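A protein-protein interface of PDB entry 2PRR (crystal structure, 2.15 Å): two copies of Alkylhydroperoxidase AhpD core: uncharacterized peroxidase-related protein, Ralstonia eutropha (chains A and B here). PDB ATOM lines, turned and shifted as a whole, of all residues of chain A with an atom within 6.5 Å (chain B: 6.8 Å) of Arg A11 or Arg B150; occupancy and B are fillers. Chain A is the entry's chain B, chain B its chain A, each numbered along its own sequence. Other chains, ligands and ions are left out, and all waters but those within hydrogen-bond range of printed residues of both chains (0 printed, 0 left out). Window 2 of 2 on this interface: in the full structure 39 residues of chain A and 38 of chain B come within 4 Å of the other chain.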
ATOM      1  N   PRO A   8     -10.188 -32.809 -19.836  1.00  0.00           N
ATOM      2  CA  PRO A   8     -11.287 -33.081 -20.749  1.00  0.00           C
ATOM      3  C   PRO A   8     -11.227 -32.118 -21.937  1.00  0.00           C
ATOM      4  O   PRO A   8     -10.791 -30.978 -21.782  1.00  0.00           O
ATOM      5  CB  PRO A   8     -12.534 -32.852 -19.889  1.00  0.00           C
ATOM      6  CG  PRO A   8     -12.099 -31.998 -18.785  1.00  0.00           C
ATOM      7  CD  PRO A   8     -10.661 -32.352 -18.518  1.00  0.00           C
ATOM      8  N   ILE A   9     -11.600 -32.608 -23.115  1.00  0.00           N
ATOM      9  CA  ILE A   9     -11.559 -31.815 -24.345  1.00  0.00           C
ATOM     10  C   ILE A   9     -12.926 -31.203 -24.695  1.00  0.00           C
ATOM     11  O   ILE A   9     -13.042 -30.425 -25.630  1.00  0.00           O
ATOM     12  CB  ILE A   9     -11.044 -32.640 -25.534  1.00  0.00           C
ATOM     13  CG1 ILE A   9     -12.018 -33.772 -25.919  1.00  0.00           C
ATOM     14  CG2 ILE A   9      -9.683 -33.230 -25.200  1.00  0.00           C
ATOM     15  CD1 ILE A   9     -11.841 -34.315 -27.333  1.00  0.00           C
ATOM     16  N   SER A  10     -13.957 -31.597 -23.961  1.00  0.00           N
ATOM     17  CA  SER A  10     -15.303 -31.101 -24.194  1.00  0.00           C
ATOM     18  C   SER A  10     -16.037 -31.235 -22.892  1.00  0.00           C
ATOM     19  O   SER A  10     -15.603 -31.936 -21.984  1.00  0.00           O
ATOM     20  CB  SER A  10     -15.998 -31.923 -25.263  1.00  0.00           C
ATOM     21  OG  SER A  10     -17.342 -31.496 -25.464  1.00  0.00           O
ATOM     22  N   ARG A  11     -17.130 -30.503 -22.788  1.00  0.00           N
ATOM     23  CA  ARG A  11     -18.005 -30.552 -21.645  1.00  0.00           C
ATOM     24  C   ARG A  11     -19.026 -31.685 -21.879  1.00  0.00           C
ATOM     25  O   ARG A  11     -19.708 -32.140 -20.967  1.00  0.00           O
ATOM     26  CB  ARG A  11     -18.708 -29.207 -21.552  1.00  0.00           C
ATOM     27  CG  ARG A  11     -19.608 -29.079 -20.404  1.00  0.00           C
ATOM     28  CD  ARG A  11     -20.519 -27.876 -20.513  1.00  0.00           C
ATOM     29  NE  ARG A  11     -21.521 -27.971 -19.464  1.00  0.00           N
ATOM     30  CZ  ARG A  11     -22.607 -28.725 -19.538  1.00  0.00           C
ATOM     31  NH1 ARG A  11     -22.876 -29.452 -20.620  1.00  0.00           N
ATOM     32  NH2 ARG A  11     -23.444 -28.741 -18.516  1.00  0.00           N
ATOM     33  N   TYR A  12     -19.126 -32.115 -23.126  1.00  0.00           N
ATOM     34  CA  TYR A  12     -20.033 -33.150 -23.546  1.00  0.00           C
ATOM     35  C   TYR A  12     -19.271 -34.457 -23.808  1.00  0.00           C
ATOM     36  O   TYR A  12     -18.050 -34.488 -23.738  1.00  0.00           O
ATOM     37  CB  TYR A  12     -20.731 -32.667 -24.801  1.00  0.00           C
ATOM     38  CG  TYR A  12     -21.822 -31.663 -24.524  1.00  0.00           C
ATOM     39  CD1 TYR A  12     -21.538 -30.327 -24.326  1.00  0.00           C
ATOM     40  CD2 TYR A  12     -23.140 -32.061 -24.476  1.00  0.00           C
ATOM     41  CE1 TYR A  12     -22.543 -29.408 -24.080  1.00  0.00           C
ATOM     42  CE2 TYR A  12     -24.154 -31.158 -24.244  1.00  0.00           C
ATOM     43  CZ  TYR A  12     -23.857 -29.835 -24.033  1.00  0.00           C
ATOM     44  OH  TYR A  12     -24.890 -28.944 -23.792  1.00  0.00           O
ATOM     45  N   PRO A  13     -19.993 -35.557 -24.029  1.00  0.00           N
ATOM     46  CA  PRO A  13     -19.339 -36.805 -24.370  1.00  0.00           C
ATOM     47  C   PRO A  13     -18.511 -36.743 -25.655  1.00  0.00           C
ATOM     48  O   PRO A  13     -18.858 -36.015 -26.591  1.00  0.00           O
ATOM     49  CB  PRO A  13     -20.519 -37.749 -24.607  1.00  0.00           C
ATOM     50  CG  PRO A  13     -21.603 -37.191 -23.803  1.00  0.00           C
ATOM     51  CD  PRO A  13     -21.449 -35.726 -23.903  1.00  0.00           C
ATOM     52  N   THR A 178     -19.124 -22.654 -26.311  1.00  0.00           N
ATOM     53  CA  THR A 178     -20.190 -23.246 -25.522  1.00  0.00           C
ATOM     54  C   THR A 178     -19.809 -24.604 -24.870  1.00  0.00           C
ATOM     55  O   THR A 178     -20.162 -24.860 -23.719  1.00  0.00           O
ATOM     56  CB  THR A 178     -21.434 -23.349 -26.327  1.00  0.00           C
ATOM     57  OG1 THR A 178     -21.870 -22.030 -26.691  1.00  0.00           O
ATOM     58  CG2 THR A 178     -22.532 -24.003 -25.523  1.00  0.00           C
ATOM     59  N   ILE A 179     -19.087 -25.460 -25.582  1.00  0.00           N
ATOM     60  CA  ILE A 179     -18.727 -26.777 -25.027  1.00  0.00           C
ATOM     61  C   ILE A 179     -17.352 -26.834 -24.419  1.00  0.00           C
ATOM     62  O   ILE A 179     -16.913 -27.899 -23.997  1.00  0.00           O
ATOM     63  CB  ILE A 179     -18.864 -27.905 -26.080  1.00  0.00           C
ATOM     64  CG1 ILE A 179     -17.634 -27.971 -27.018  1.00  0.00           C
ATOM     65  CG2 ILE A 179     -20.208 -27.747 -26.836  1.00  0.00           C
ATOM     66  CD1 ILE A 179     -17.737 -29.040 -28.090  1.00  0.00           C
ATOM     67  N   GLY A 180     -16.646 -25.717 -24.366  1.00  0.00           N
ATOM     68  CA  GLY A 180     -15.324 -25.730 -23.755  1.00  0.00           C
ATOM     69  C   GLY A 180     -14.368 -26.610 -24.525  1.00  0.00           C
ATOM     70  O   GLY A 180     -13.586 -27.364 -23.928  1.00  0.00           O
ATOM     71  N   MET A 181     -14.401 -26.448 -25.854  1.00  0.00           N
ATOM     72  CA  MET A 181     -13.585 -27.224 -26.771  1.00  0.00           C
ATOM     73  C   MET A 181     -12.101 -26.963 -26.502  1.00  0.00           C
ATOM     74  O   MET A 181     -11.616 -25.840 -26.618  1.00  0.00           O
ATOM     75  CB  MET A 181     -13.922 -26.862 -28.202  1.00  0.00           C
ATOM     76  CG  MET A 181     -13.607 -27.938 -29.150  1.00  0.00           C
ATOM     77  SD  MET A 181     -13.658 -27.430 -30.894  1.00  0.00           S
ATOM     78  CE  MET A 181     -15.712 -27.489 -31.245  1.00  0.00           C
ATOM     79  N   VAL B 141     -19.569 -18.486 -21.286  1.00  0.00           N
ATOM     80  CA  VAL B 141     -20.507 -19.551 -20.973  1.00  0.00           C
ATOM     81  C   VAL B 141     -19.848 -20.477 -19.929  1.00  0.00           C
ATOM     82  O   VAL B 141     -18.728 -20.906 -20.131  1.00  0.00           O
ATOM     83  CB  VAL B 141     -20.913 -20.314 -22.236  1.00  0.00           C
ATOM     84  CG1 VAL B 141     -21.459 -21.650 -21.888  1.00  0.00           C
ATOM     85  CG2 VAL B 141     -21.963 -19.495 -23.085  1.00  0.00           C
ATOM     86  N   ASN B 142     -20.556 -20.714 -18.822  1.00  0.00           N
ATOM     87  CA  ASN B 142     -20.121 -21.529 -17.682  1.00  0.00           C
ATOM     88  C   ASN B 142     -21.212 -22.515 -17.200  1.00  0.00           C
ATOM     89  O   ASN B 142     -22.328 -22.537 -17.732  1.00  0.00           O
ATOM     90  CB  ASN B 142     -19.619 -20.625 -16.523  1.00  0.00           C
ATOM     91  CG  ASN B 142     -20.616 -19.547 -16.120  1.00  0.00           C
ATOM     92  OD1 ASN B 142     -21.806 -19.794 -15.917  1.00  0.00           O
ATOM     93  ND2 ASN B 142     -20.112 -18.337 -15.980  1.00  0.00           N
ATOM     94  N   GLU B 143     -20.874 -23.323 -16.193  1.00  0.00           N
ATOM     95  CA  GLU B 143     -21.804 -24.308 -15.619  1.00  0.00           C
ATOM     96  C   GLU B 143     -23.067 -23.714 -14.992  1.00  0.00           C
ATOM     97  O   GLU B 143     -24.122 -24.344 -14.985  1.00  0.00           O
ATOM     98  CB  GLU B 143     -21.082 -25.167 -14.576  1.00  0.00           C
ATOM     99  CG  GLU B 143     -20.020 -26.083 -15.179  1.00  0.00           C
ATOM    100  CD  GLU B 143     -20.619 -27.138 -16.107  1.00  0.00           C
ATOM    101  OE1 GLU B 143     -21.699 -27.675 -15.766  1.00  0.00           O
ATOM    102  OE2 GLU B 143     -20.008 -27.434 -17.163  1.00  0.00           O
ATOM    103  N   ALA B 144     -22.967 -22.513 -14.466  1.00  0.00           N
ATOM    104  CA  ALA B 144     -24.110 -21.862 -13.889  1.00  0.00           C
ATOM    105  C   ALA B 144     -25.117 -21.521 -14.980  1.00  0.00           C
ATOM    106  O   ALA B 144     -26.287 -21.387 -14.695  1.00  0.00           O
ATOM    107  CB  ALA B 144     -23.688 -20.636 -13.166  1.00  0.00           C
ATOM    108  N   ASP B 145     -24.661 -21.380 -16.226  1.00  0.00           N
ATOM    109  CA  ASP B 145     -25.550 -21.118 -17.364  1.00  0.00           C
ATOM    110  C   ASP B 145     -26.437 -22.328 -17.680  1.00  0.00           C
ATOM    111  O   ASP B 145     -27.633 -22.171 -17.974  1.00  0.00           O
ATOM    112  CB  ASP B 145     -24.738 -20.708 -18.599  1.00  0.00           C
ATOM    113  CG  ASP B 145     -24.057 -19.367 -18.442  1.00  0.00           C
ATOM    114  OD1 ASP B 145     -24.777 -18.384 -18.175  1.00  0.00           O
ATOM    115  OD2 ASP B 145     -22.812 -19.284 -18.630  1.00  0.00           O
ATOM    116  N   PHE B 146     -25.819 -23.513 -17.618  1.00  0.00           N
ATOM    117  CA  PHE B 146     -26.471 -24.801 -17.847  1.00  0.00           C
ATOM    118  C   PHE B 146     -27.379 -25.143 -16.689  1.00  0.00           C
ATOM    119  O   PHE B 146     -28.500 -25.647 -16.890  1.00  0.00           O
ATOM    120  CB  PHE B 146     -25.435 -25.927 -18.088  1.00  0.00           C
ATOM    121  CG  PHE B 146     -24.678 -25.768 -19.371  1.00  0.00           C
ATOM    122  CD1 PHE B 146     -25.213 -26.227 -20.570  1.00  0.00           C
ATOM    123  CD2 PHE B 146     -23.430 -25.127 -19.393  1.00  0.00           C
ATOM    124  CE1 PHE B 146     -24.533 -26.028 -21.777  1.00  0.00           C
ATOM    125  CE2 PHE B 146     -22.734 -24.954 -20.585  1.00  0.00           C
ATOM    126  CZ  PHE B 146     -23.291 -25.397 -21.783  1.00  0.00           C
ATOM    127  N   GLU B 147     -26.893 -24.870 -15.479  1.00  0.00           N
ATOM    128  CA  GLU B 147     -27.702 -25.042 -14.272  1.00  0.00           C
ATOM    129  C   GLU B 147     -28.986 -24.246 -14.353  1.00  0.00           C
ATOM    130  O   GLU B 147     -30.031 -24.787 -14.022  1.00  0.00           O
ATOM    131  CB  GLU B 147     -26.949 -24.657 -13.014  1.00  0.00           C
ATOM    132  CG  GLU B 147     -25.970 -25.731 -12.571  1.00  0.00           C
ATOM    133  CD  GLU B 147     -25.103 -25.321 -11.405  1.00  0.00           C
ATOM    134  OE1 GLU B 147     -25.502 -24.398 -10.646  1.00  0.00           O
ATOM    135  OE2 GLU B 147     -24.022 -25.947 -11.254  1.00  0.00           O
ATOM    136  N   ALA B 148     -28.925 -22.986 -14.782  1.00  0.00           N
ATOM    137  CA  ALA B 148     -30.159 -22.176 -14.920  1.00  0.00           C
ATOM    138  C   ALA B 148     -31.138 -22.775 -15.906  1.00  0.00           C
ATOM    139  O   ALA B 148     -32.355 -22.693 -15.727  1.00  0.00           O
ATOM    140  CB  ALA B 148     -29.834 -20.781 -15.358  1.00  0.00           C
ATOM    141  N   LEU B 149     -30.603 -23.331 -16.987  1.00  0.00           N
ATOM    142  CA  LEU B 149     -31.422 -23.935 -18.035  1.00  0.00           C
ATOM    143  C   LEU B 149     -32.165 -25.180 -17.561  1.00  0.00           C
ATOM    144  O   LEU B 149     -33.350 -25.338 -17.839  1.00  0.00           O
ATOM    145  CB  LEU B 149     -30.549 -24.284 -19.244  1.00  0.00           C
ATOM    146  CG  LEU B 149     -30.136 -23.153 -20.161  1.00  0.00           C
ATOM    147  CD1 LEU B 149     -29.125 -23.710 -21.145  1.00  0.00           C
ATOM    148  CD2 LEU B 149     -31.368 -22.541 -20.892  1.00  0.00           C
ATOM    149  N   ARG B 150     -31.440 -26.051 -16.863  1.00  0.00           N
ATOM    150  CA  ARG B 150     -31.972 -27.282 -16.301  1.00  0.00           C
ATOM    151  C   ARG B 150     -33.167 -27.083 -15.403  1.00  0.00           C
ATOM    152  O   ARG B 150     -34.040 -27.925 -15.374  1.00  0.00           O
ATOM    153  CB  ARG B 150     -30.886 -28.031 -15.516  1.00  0.00           C
ATOM    154  CG  ARG B 150     -29.830 -28.647 -16.407  1.00  0.00           C
ATOM    155  CD  ARG B 150     -28.999 -29.695 -15.680  1.00  0.00           C
ATOM    156  NE  ARG B 150     -27.949 -29.143 -14.828  1.00  0.00           N
ATOM    157  CZ  ARG B 150     -26.664 -28.986 -15.170  1.00  0.00           C
ATOM    158  NH1 ARG B 150     -26.207 -29.327 -16.368  1.00  0.00           N
ATOM    159  NH2 ARG B 150     -25.817 -28.476 -14.290  1.00  0.00           N
ATOM    160  N   GLU B 151     -33.181 -25.980 -14.662  1.00  0.00           N
ATOM    161  CA  GLU B 151     -34.281 -25.613 -13.772  1.00  0.00           C
ATOM    162  C   GLU B 151     -35.608 -25.487 -14.527  1.00  0.00           C
ATOM    163  O   GLU B 151     -36.647 -25.686 -13.931  1.00  0.00           O
ATOM    164  CB  GLU B 151     -33.968 -24.285 -13.060  1.00  0.00           C
ATOM    165  CG  GLU B 151     -32.810 -24.379 -12.055  1.00  0.00           C
ATOM    166  CD  GLU B 151     -33.255 -24.684 -10.628  1.00  0.00           C
ATOM    167  OE1 GLU B 151     -33.637 -23.715  -9.930  1.00  0.00           O
ATOM    168  OE2 GLU B 151     -33.171 -25.864 -10.192  1.00  0.00           O
ATOM    169  N   HIS B 152     -35.543 -25.162 -15.820  1.00  0.00           N
ATOM    170  CA  HIS B 152     -36.728 -24.999 -16.700  1.00  0.00           C
ATOM    171  C   HIS B 152     -37.089 -26.187 -17.601  1.00  0.00           C
ATOM    172  O   HIS B 152     -38.048 -26.099 -18.394  1.00  0.00           O
ATOM    173  CB  HIS B 152     -36.531 -23.747 -17.563  1.00  0.00           C
ATOM    174  CG  HIS B 152     -36.519 -22.505 -16.757  1.00  0.00           C
ATOM    175  ND1 HIS B 152     -37.671 -21.952 -16.235  1.00  0.00           N
ATOM    176  CD2 HIS B 152     -35.493 -21.756 -16.295  1.00  0.00           C
ATOM    177  CE1 HIS B 152     -37.354 -20.890 -15.519  1.00  0.00           C
ATOM    178  NE2 HIS B 152     -36.036 -20.752 -15.536  1.00  0.00           N
ATOM    179  N   GLY B 153     -36.305 -27.268 -17.491  1.00  0.00           N
ATOM    180  CA  GLY B 153     -36.533 -28.483 -18.228  1.00  0.00           C
ATOM    181  C   GLY B 153     -35.657 -28.737 -19.429  1.00  0.00           C
ATOM    182  O   GLY B 153     -35.918 -29.659 -20.197  1.00  0.00           O
ATOM    183  N   PHE B 154     -34.610 -27.936 -19.603  1.00  0.00           N
ATOM    184  CA  PHE B 154     -33.690 -28.116 -20.720  1.00  0.00           C
ATOM    185  C   PHE B 154     -32.518 -29.018 -20.282  1.00  0.00           C
ATOM    186  O   PHE B 154     -31.789 -28.689 -19.360  1.00  0.00           O
ATOM    187  CB  PHE B 154     -33.145 -26.763 -21.209  1.00  0.00           C
ATOM    188  CG  PHE B 154     -34.220 -25.804 -21.728  1.00  0.00           C
ATOM    189  CD1 PHE B 154     -34.800 -25.999 -22.964  1.00  0.00           C
ATOM    190  CD2 PHE B 154     -34.573 -24.676 -21.000  1.00  0.00           C
ATOM    191  CE1 PHE B 154     -35.806 -25.113 -23.454  1.00  0.00           C
ATOM    192  CE2 PHE B 154     -35.534 -23.783 -21.485  1.00  0.00           C
ATOM    193  CZ  PHE B 154     -36.166 -24.024 -22.707  1.00  0.00           C
ATOM    194  N   THR B 155     -32.341 -30.143 -20.952  1.00  0.00           N
ATOM    195  CA  THR B 155     -31.200 -31.038 -20.676  1.00  0.00           C
ATOM    196  C   THR B 155     -29.941 -30.427 -21.274  1.00  0.00           C
ATOM    197  O   THR B 155     -30.003 -29.404 -21.943  1.00  0.00           O
ATOM    198  CB  THR B 155     -31.435 -32.428 -21.299  1.00  0.00           C
ATOM    199  OG1 THR B 155     -31.494 -32.335 -22.732  1.00  0.00           O
ATOM    200  CG2 THR B 155     -32.749 -33.002 -20.793  1.00  0.00           C
ATOM    201  N   ASP B 156     -28.795 -31.050 -21.051  1.00  0.00           N
ATOM    202  CA  ASP B 156     -27.562 -30.548 -21.624  1.00  0.00           C
ATOM    203  C   ASP B 156     -27.619 -30.704 -23.117  1.00  0.00           C
ATOM    204  O   ASP B 156     -27.060 -29.899 -23.846  1.00  0.00           O
ATOM    205  CB  ASP B 156     -26.354 -31.264 -21.022  1.00  0.00           C
ATOM    206  CG  ASP B 156     -26.238 -31.010 -19.543  1.00  0.00           C
ATOM    207  OD1 ASP B 156     -26.508 -29.874 -19.102  1.00  0.00           O
ATOM    208  OD2 ASP B 156     -25.924 -31.950 -18.801  1.00  0.00           O
ATOM    209  N   GLU B 157     -28.316 -31.736 -23.576  1.00  0.00           N
ATOM    210  CA  GLU B 157     -28.517 -31.938 -25.001  1.00  0.00           C
ATOM    211  C   GLU B 157     -29.460 -30.869 -25.573  1.00  0.00           C
ATOM    212  O   GLU B 157     -29.343 -30.514 -26.723  1.00  0.00           O
ATOM    213  CB  GLU B 157     -29.019 -33.351 -25.292  1.00  0.00           C
ATOM    214  CG  GLU B 157     -28.019 -34.441 -24.919  1.00  0.00           C
ATOM    215  CD  GLU B 157     -26.697 -34.339 -25.666  1.00  0.00           C
ATOM    216  OE1 GLU B 157     -26.713 -34.209 -26.905  1.00  0.00           O
ATOM    217  OE2 GLU B 157     -25.640 -34.407 -25.006  1.00  0.00           O
ATOM    218  N   ALA B 159     -29.522 -27.722 -24.249  1.00  0.00           N
ATOM    219  CA  ALA B 159     -28.670 -26.551 -24.222  1.00  0.00           C
ATOM    220  C   ALA B 159     -27.793 -26.519 -25.475  1.00  0.00           C
ATOM    221  O   ALA B 159     -27.614 -25.446 -26.066  1.00  0.00           O
ATOM    222  CB  ALA B 159     -27.798 -26.522 -22.960  1.00  0.00           C
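NH1 of Arg B150 lies within salt-bridge range of OD1 of Asp B156 (2.8 Å).
The backbone NH (N) of Glu B157 sits close to the side-chain hydroxyl (OG1) of Thr B155 (3.3 Å).
The side-chain hydroxyl of Ser A10 is in hydrogen-bond range of the backbone NH of Tyr A12 (3.0 Å).
The backbone NH (N) of Arg A11 is in hydrogen-bond range of the backbone carbonyl oxygen (O) of Ile A179.
Hydrophobic or aromatic side chains of chain B within 4 Å of the printed part of chain A: Val B141, Phe B146 and Ala B159.
Among the printed residues, Asp or Glu carboxylates within 4 Å of a Lys or Arg side-chain nitrogen of the other chain: Arg A11 with Glu B143 (2.8 Å) and Arg A11 with Asp B156 (3.3 Å).
The guanidinium group of Arg A11 lies within salt-bridge range of the side-chain carboxylate of Glu B143 (2.8 Å).
The side-chain carboxylate (OD1) of Asp B156 lies within salt-bridge range of the guanidinium group (NH2) of Arg A11, at 3.3 Å.
OH of Tyr A12 sits close to O of Asp B156 (2.4 Å).
Arg A11 touches just these residues of chain B: Glu B143, Phe B146, Arg B150 and Asp B156.
Arg B150 touches just one residue of chain A: Arg A11 (3.5 Å).
Of the printed residues of chain A, Phe B146 touches Arg A11 (3.3 Å), Tyr A12 (3.6 Å) and Thr A178 (3.7 Å).
Of the printed residues of chain A, Ala B159 touches Tyr A12.
Of the printed residues of chain A, Asp B156 touches Arg A11 (3.3 Å) and Tyr A12 (2.4 Å).
Ser A10 touches none of the printed residues of chain B.
Among the printed residues, merely in contact across the chains: Arg A11 with Phe B146, Tyr A12 with Glu B157, Arg A11 with Arg B150, Tyr A12 with Phe B146, Thr A178 with Phe B146, Tyr A12 with Ala B159 and Thr A178 with Val B141.
No position is printed for both chains.
Of the 10 pairs that touch across the chains among the printed residues, none has its exchanged pair printed and touching as well.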
